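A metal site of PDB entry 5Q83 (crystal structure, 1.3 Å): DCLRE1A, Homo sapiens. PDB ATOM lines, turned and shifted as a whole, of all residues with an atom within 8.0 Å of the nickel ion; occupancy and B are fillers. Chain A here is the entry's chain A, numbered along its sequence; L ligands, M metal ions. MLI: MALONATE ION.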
ATOM      1  N   ASP A  18      18.833 -12.026  18.491  1.00  0.00           N
ATOM      2  CA  ASP A  18      18.231 -12.651  19.699  1.00  0.00           C
ATOM      3  C   ASP A  18      19.092 -13.923  20.141  1.00  0.00           C
ATOM      4  O   ASP A  18      18.529 -14.994  20.462  1.00  0.00           O
ATOM      5  CB  ASP A  18      16.788 -12.970  19.523  1.00  0.00           C
ATOM      6  CG  ASP A  18      15.925 -11.711  19.204  1.00  0.00           C
ATOM      7  OD1 ASP A  18      16.446 -10.620  19.446  1.00  0.00           O
ATOM      8  OD2 ASP A  18      14.738 -11.951  18.801  1.00  0.00           O
ATOM      9  N   THR A  34      15.548  -7.922  19.215  1.00  0.00           N
ATOM     10  CA  THR A  34      14.303  -7.437  18.619  1.00  0.00           C
ATOM     11  C   THR A  34      13.352  -6.848  19.686  1.00  0.00           C
ATOM     12  O   THR A  34      12.597  -5.890  19.347  1.00  0.00           O
ATOM     13  CB  THR A  34      13.564  -8.497  17.790  1.00  0.00           C
ATOM     14  OG1 THR A  34      13.217  -9.638  18.676  1.00  0.00           O
ATOM     15  CG2 THR A  34      14.418  -9.024  16.644  1.00  0.00           C
ATOM     16  N   HIS A  35      13.322  -7.422  20.900  1.00  0.00           N
ATOM     17  CA  HIS A  35      12.358  -6.983  21.950  1.00  0.00           C
ATOM     18  C   HIS A  35      12.777  -7.536  23.288  1.00  0.00           C
ATOM     19  O   HIS A  35      13.468  -8.587  23.346  1.00  0.00           O
ATOM     20  CB  HIS A  35      10.896  -7.331  21.549  1.00  0.00           C
ATOM     21  CG  HIS A  35      10.541  -8.785  21.517  1.00  0.00           C
ATOM     22  ND1 HIS A  35      10.984  -9.710  20.564  1.00  0.00           N
ATOM     23  CD2 HIS A  35       9.663  -9.466  22.277  1.00  0.00           C
ATOM     24  CE1 HIS A  35      10.404 -10.885  20.824  1.00  0.00           C
ATOM     25  NE2 HIS A  35       9.601 -10.742  21.825  1.00  0.00           N
ATOM     26  N   PHE A  36      12.228  -6.951  24.321  1.00  0.00           N
ATOM     27  CA  PHE A  36      12.546  -7.339  25.696  1.00  0.00           C
ATOM     28  C   PHE A  36      11.602  -8.422  26.257  1.00  0.00           C
ATOM     29  O   PHE A  36      10.777  -8.132  27.210  1.00  0.00           O
ATOM     30  CB  PHE A  36      12.530  -6.053  26.615  1.00  0.00           C
ATOM     31  CG  PHE A  36      13.175  -6.228  28.000  1.00  0.00           C
ATOM     32  CD1 PHE A  36      14.549  -6.241  28.078  1.00  0.00           C
ATOM     33  CD2 PHE A  36      12.410  -6.414  29.146  1.00  0.00           C
ATOM     34  CE1 PHE A  36      15.192  -6.400  29.327  1.00  0.00           C
ATOM     35  CE2 PHE A  36      13.025  -6.551  30.388  1.00  0.00           C
ATOM     36  CZ  PHE A  36      14.367  -6.514  30.490  1.00  0.00           C
ATOM     37  N   HIS A  37      11.652  -9.643  25.697  1.00  0.00           N
ATOM     38  CA  HIS A  37      11.007 -10.846  26.246  1.00  0.00           C
ATOM     39  C   HIS A  37      12.120 -11.858  26.560  1.00  0.00           C
ATOM     40  O   HIS A  37      13.115 -11.958  25.814  1.00  0.00           O
ATOM     41  CB  HIS A  37       9.951 -11.506  25.311  1.00  0.00           C
ATOM     42  CG  HIS A  37       8.615 -10.804  25.290  1.00  0.00           C
ATOM     43  ND1 HIS A  37       7.671 -11.001  24.312  1.00  0.00           N
ATOM     44  CD2 HIS A  37       8.040  -9.988  26.192  1.00  0.00           C
ATOM     45  CE1 HIS A  37       6.563 -10.346  24.599  1.00  0.00           C
ATOM     46  NE2 HIS A  37       6.793  -9.668  25.713  1.00  0.00           N
ATOM     47  N   SER A  38      11.952 -12.604  27.683  1.00  0.00           N
ATOM     48  CA  SER A  38      13.070 -13.373  28.301  1.00  0.00           C
ATOM     49  C   SER A  38      13.591 -14.425  27.328  1.00  0.00           C
ATOM     50  O   SER A  38      14.823 -14.614  27.331  1.00  0.00           O
ATOM     51  CB  SER A  38      12.691 -13.907  29.697  1.00  0.00           C
ATOM     52  OG  SER A  38      11.600 -14.751  29.578  1.00  0.00           O
ATOM     53  N   ASP A  39      12.760 -15.107  26.535  1.00  0.00           N
ATOM     54  CA  ASP A  39      13.298 -16.179  25.622  1.00  0.00           C
ATOM     55  C   ASP A  39      14.247 -15.544  24.610  1.00  0.00           C
ATOM     56  O   ASP A  39      15.039 -16.271  23.961  1.00  0.00           O
ATOM     57  CB  ASP A  39      12.187 -16.861  24.894  1.00  0.00           C
ATOM     58  CG  ASP A  39      11.483 -18.038  25.716  1.00  0.00           C
ATOM     59  OD1 ASP A  39      11.908 -18.280  26.847  1.00  0.00           O
ATOM     60  OD2 ASP A  39      10.511 -18.625  25.159  1.00  0.00           O
ATOM     61  N   HIS A  40      14.116 -14.227  24.348  1.00  0.00           N
ATOM     62  CA  HIS A  40      14.996 -13.513  23.413  1.00  0.00           C
ATOM     63  C   HIS A  40      16.141 -12.821  23.987  1.00  0.00           C
ATOM     64  O   HIS A  40      17.239 -12.828  23.348  1.00  0.00           O
ATOM     65  CB  HIS A  40      14.033 -12.498  22.604  1.00  0.00           C
ATOM     66  CG  HIS A  40      12.966 -13.191  21.871  1.00  0.00           C
ATOM     67  ND1 HIS A  40      12.990 -13.429  20.514  1.00  0.00           N
ATOM     68  CD2 HIS A  40      11.789 -13.725  22.273  1.00  0.00           C
ATOM     69  CE1 HIS A  40      11.942 -14.114  20.134  1.00  0.00           C
ATOM     70  NE2 HIS A  40      11.184 -14.313  21.212  1.00  0.00           N
ATOM     71  N   HIS A  96       4.046  -5.842  18.246  1.00  0.00           N
ATOM     72  CA  HIS A  96       4.170  -6.916  19.280  1.00  0.00           C
ATOM     73  C   HIS A  96       4.025  -6.229  20.605  1.00  0.00           C
ATOM     74  O   HIS A  96       2.882  -5.661  20.850  1.00  0.00           O
ATOM     75  CB  HIS A  96       5.431  -7.761  19.047  1.00  0.00           C
ATOM     76  CG  HIS A  96       5.660  -8.945  19.966  1.00  0.00           C
ATOM     77  ND1 HIS A  96       4.713  -9.922  20.127  1.00  0.00           N
ATOM     78  CD2 HIS A  96       6.693  -9.292  20.775  1.00  0.00           C
ATOM     79  CE1 HIS A  96       5.195 -10.851  20.972  1.00  0.00           C
ATOM     80  NE2 HIS A  96       6.418 -10.533  21.361  1.00  0.00           N
ATOM     81  N   CYS A  97       5.013  -6.209  21.482  1.00  0.00           N
ATOM     82  CA  CYS A  97       4.999  -5.462  22.778  1.00  0.00           C
ATOM     83  C   CYS A  97       5.730  -4.135  22.608  1.00  0.00           C
ATOM     84  O   CYS A  97       6.357  -3.905  21.569  1.00  0.00           O
ATOM     85  CB  CYS A  97       5.668  -6.378  23.851  1.00  0.00           C
ATOM     86  SG  CYS A  97       7.470  -6.703  23.503  1.00  0.00           S
ATOM     87  N   ALA A 100       9.203  -3.448  20.456  1.00  0.00           N
ATOM     88  CA  ALA A 100       9.514  -4.549  19.564  1.00  0.00           C
ATOM     89  C   ALA A 100       9.623  -4.096  18.112  1.00  0.00           C
ATOM     90  O   ALA A 100       8.798  -3.328  17.626  1.00  0.00           O
ATOM     91  CB  ALA A 100       8.467  -5.618  19.679  1.00  0.00           C
ATOM     92  N   GLY A 117      11.409 -10.624  13.955  1.00  0.00           N
ATOM     93  CA  GLY A 117      11.352 -10.830  15.395  1.00  0.00           C
ATOM     94  C   GLY A 117      10.044 -11.519  15.729  1.00  0.00           C
ATOM     95  O   GLY A 117       9.580 -12.382  14.960  1.00  0.00           O
ATOM     96  N   ASP A 118       9.449 -11.168  16.876  1.00  0.00           N
ATOM     97  CA  ASP A 118       8.021 -11.546  17.151  1.00  0.00           C
ATOM     98  C   ASP A 118       7.115 -10.397  16.595  1.00  0.00           C
ATOM     99  O   ASP A 118       7.426  -9.209  16.789  1.00  0.00           O
ATOM    100  CB  ASP A 118       7.734 -11.741  18.621  1.00  0.00           C
ATOM    101  CG  ASP A 118       8.234 -13.059  19.233  1.00  0.00           C
ATOM    102  OD1 ASP A 118       8.596 -13.967  18.468  1.00  0.00           O
ATOM    103  OD2 ASP A 118       8.135 -13.184  20.465  1.00  0.00           O
ATOM    104  N   PHE A 119       6.059 -10.774  15.888  1.00  0.00           N
ATOM    105  CA  PHE A 119       5.164  -9.730  15.290  1.00  0.00           C
ATOM    106  C   PHE A 119       3.726 -10.147  15.194  1.00  0.00           C
ATOM    107  O   PHE A 119       3.420 -11.339  15.177  1.00  0.00           O
ATOM    108  CB  PHE A 119       5.698  -9.206  13.896  1.00  0.00           C
ATOM    109  CG  PHE A 119       5.356  -9.974  12.600  1.00  0.00           C
ATOM    110  CD1 PHE A 119       5.027  -9.314  11.425  1.00  0.00           C
ATOM    111  CD2 PHE A 119       5.343 -11.361  12.551  1.00  0.00           C
ATOM    112  CE1 PHE A 119       4.778  -9.989  10.264  1.00  0.00           C
ATOM    113  CE2 PHE A 119       5.048 -12.052  11.376  1.00  0.00           C
ATOM    114  CZ  PHE A 119       4.766 -11.343  10.229  1.00  0.00           C
ATOM    115  N   ASP A 141       8.272 -15.101  12.209  1.00  0.00           N
ATOM    116  CA  ASP A 141       7.562 -15.542  13.469  1.00  0.00           C
ATOM    117  C   ASP A 141       6.366 -16.346  13.051  1.00  0.00           C
ATOM    118  O   ASP A 141       5.324 -15.865  12.664  1.00  0.00           O
ATOM    119  CB  ASP A 141       7.167 -14.345  14.329  1.00  0.00           C
ATOM    120  CG  ASP A 141       6.186 -14.660  15.426  1.00  0.00           C
ATOM    121  OD1 ASP A 141       6.053 -15.874  15.752  1.00  0.00           O
ATOM    122  OD2 ASP A 141       5.584 -13.743  15.976  1.00  0.00           O
ATOM    123  N   THR A 143       4.715 -18.538  15.114  1.00  0.00           N
ATOM    124  CA  THR A 143       4.059 -19.035  16.348  1.00  0.00           C
ATOM    125  C   THR A 143       2.748 -19.728  16.071  1.00  0.00           C
ATOM    126  O   THR A 143       2.520 -20.886  16.536  1.00  0.00           O
ATOM    127  CB  THR A 143       3.901 -17.847  17.362  1.00  0.00           C
ATOM    128  OG1 THR A 143       5.164 -17.373  17.780  1.00  0.00           O
ATOM    129  CG2 THR A 143       3.152 -18.312  18.650  1.00  0.00           C
ATOM    130  N   SER A 183       5.193 -10.324  31.822  1.00  0.00           N
ATOM    131  CA  SER A 183       6.167  -9.764  30.894  1.00  0.00           C
ATOM    132  C   SER A 183       5.599  -8.419  30.395  1.00  0.00           C
ATOM    133  O   SER A 183       4.375  -8.158  30.552  1.00  0.00           O
ATOM    134  CB  SER A 183       6.347 -10.655  29.678  1.00  0.00           C
ATOM    135  OG  SER A 183       5.133 -10.903  28.986  1.00  0.00           O
ATOM    136  N   ILE A 184       6.352  -7.598  29.708  1.00  0.00           N
ATOM    137  CA  ILE A 184       5.768  -6.486  29.014  1.00  0.00           C
ATOM    138  C   ILE A 184       4.911  -6.943  27.869  1.00  0.00           C
ATOM    139  O   ILE A 184       5.012  -8.130  27.372  1.00  0.00           O
ATOM    140  CB  ILE A 184       6.849  -5.500  28.484  1.00  0.00           C
ATOM    141  CG1 ILE A 184       7.755  -6.073  27.394  1.00  0.00           C
ATOM    142  CG2 ILE A 184       7.630  -4.898  29.636  1.00  0.00           C
ATOM    143  CD1 ILE A 184       8.614  -5.053  26.701  1.00  0.00           C
ATOM    144  N   GLU A 296      -0.649 -10.852  20.768  1.00  0.00           N
ATOM    145  CA  GLU A 296       0.411 -10.014  20.148  1.00  0.00           C
ATOM    146  C   GLU A 296       1.279 -10.762  19.078  1.00  0.00           C
ATOM    147  O   GLU A 296       2.364 -10.336  18.702  1.00  0.00           O
ATOM    148  CB  GLU A 296       1.256  -9.267  21.167  1.00  0.00           C
ATOM    149  CG  GLU A 296       0.422  -8.185  21.968  1.00  0.00           C
ATOM    150  CD  GLU A 296       1.214  -7.320  22.932  1.00  0.00           C
ATOM    151  OE1 GLU A 296       2.325  -7.718  23.392  1.00  0.00           O
ATOM    152  OE2 GLU A 296       0.663  -6.199  23.313  1.00  0.00           O
ATOM    153  N   HIS A 297       0.713 -11.889  18.599  1.00  0.00           N
ATOM    154  CA  HIS A 297       1.240 -12.584  17.436  1.00  0.00           C
ATOM    155  C   HIS A 297       0.209 -12.726  16.318  1.00  0.00           C
ATOM    156  O   HIS A 297      -1.010 -12.758  16.580  1.00  0.00           O
ATOM    157  CB  HIS A 297       1.730 -14.067  17.816  1.00  0.00           C
ATOM    158  CG  HIS A 297       2.863 -14.155  18.766  1.00  0.00           C
ATOM    159  ND1 HIS A 297       4.184 -14.122  18.375  1.00  0.00           N
ATOM    160  CD2 HIS A 297       2.873 -14.386  20.117  1.00  0.00           C
ATOM    161  CE1 HIS A 297       4.956 -14.308  19.469  1.00  0.00           C
ATOM    162  NE2 HIS A 297       4.164 -14.411  20.502  1.00  0.00           N
HETATM  163  C1  MLI L   1       6.947 -14.504  24.394  1.00  0.00           C
HETATM  164  C2  MLI L   1       5.874 -14.229  23.346  1.00  0.00           C
HETATM  165  C3  MLI L   1       8.371 -14.572  23.782  1.00  0.00           C
HETATM  166  O6  MLI L   1       4.859 -14.914  23.132  1.00  0.00           O
HETATM  167  O7  MLI L   1       6.021 -13.250  22.654  1.00  0.00           O
HETATM  168  O8  MLI L   1       8.790 -13.639  23.097  1.00  0.00           O
HETATM  169  O9  MLI L   1       9.089 -15.582  24.142  1.00  0.00           O
HETATM  170 NI    NI M   1       7.810 -12.033  22.303  1.00  0.00          NI
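The nickel ion is bound by O8 of the ligand, O7 of the ligand, OD2 of Asp 118, NE2 of His 96, NE2 of His 35 and ND1 of His 37.
The nickel ion has six donor atoms within binding distance.
Within 4 Å of the nickel ion: His 35, His 37, His 96 and Asp 118.
Along chain A the residues within 4 Å of the nickel ion span positions 35 to 118.
A ring nitrogen (NE2) of His 40 sits close to the side-chain carboxylate of Asp 118 (3.3 Å).
A ring nitrogen (ND1) of His 96 is in hydrogen-bond range of the backbone carbonyl oxygen (O) of Glu 296, 2.8 Å away.
ND1 of His 35 sits at hydrogen-bond distance from OG1 of Thr 34 (2.9 Å).
A ring nitrogen (NE2) of His 37 is in hydrogen-bond range of the side-chain sulfur (SG) of Cys 97 (3.8 Å).
A ring nitrogen (NE2) of His 37 sits at hydrogen-bond distance from the backbone carbonyl oxygen (O) of Ile 184.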
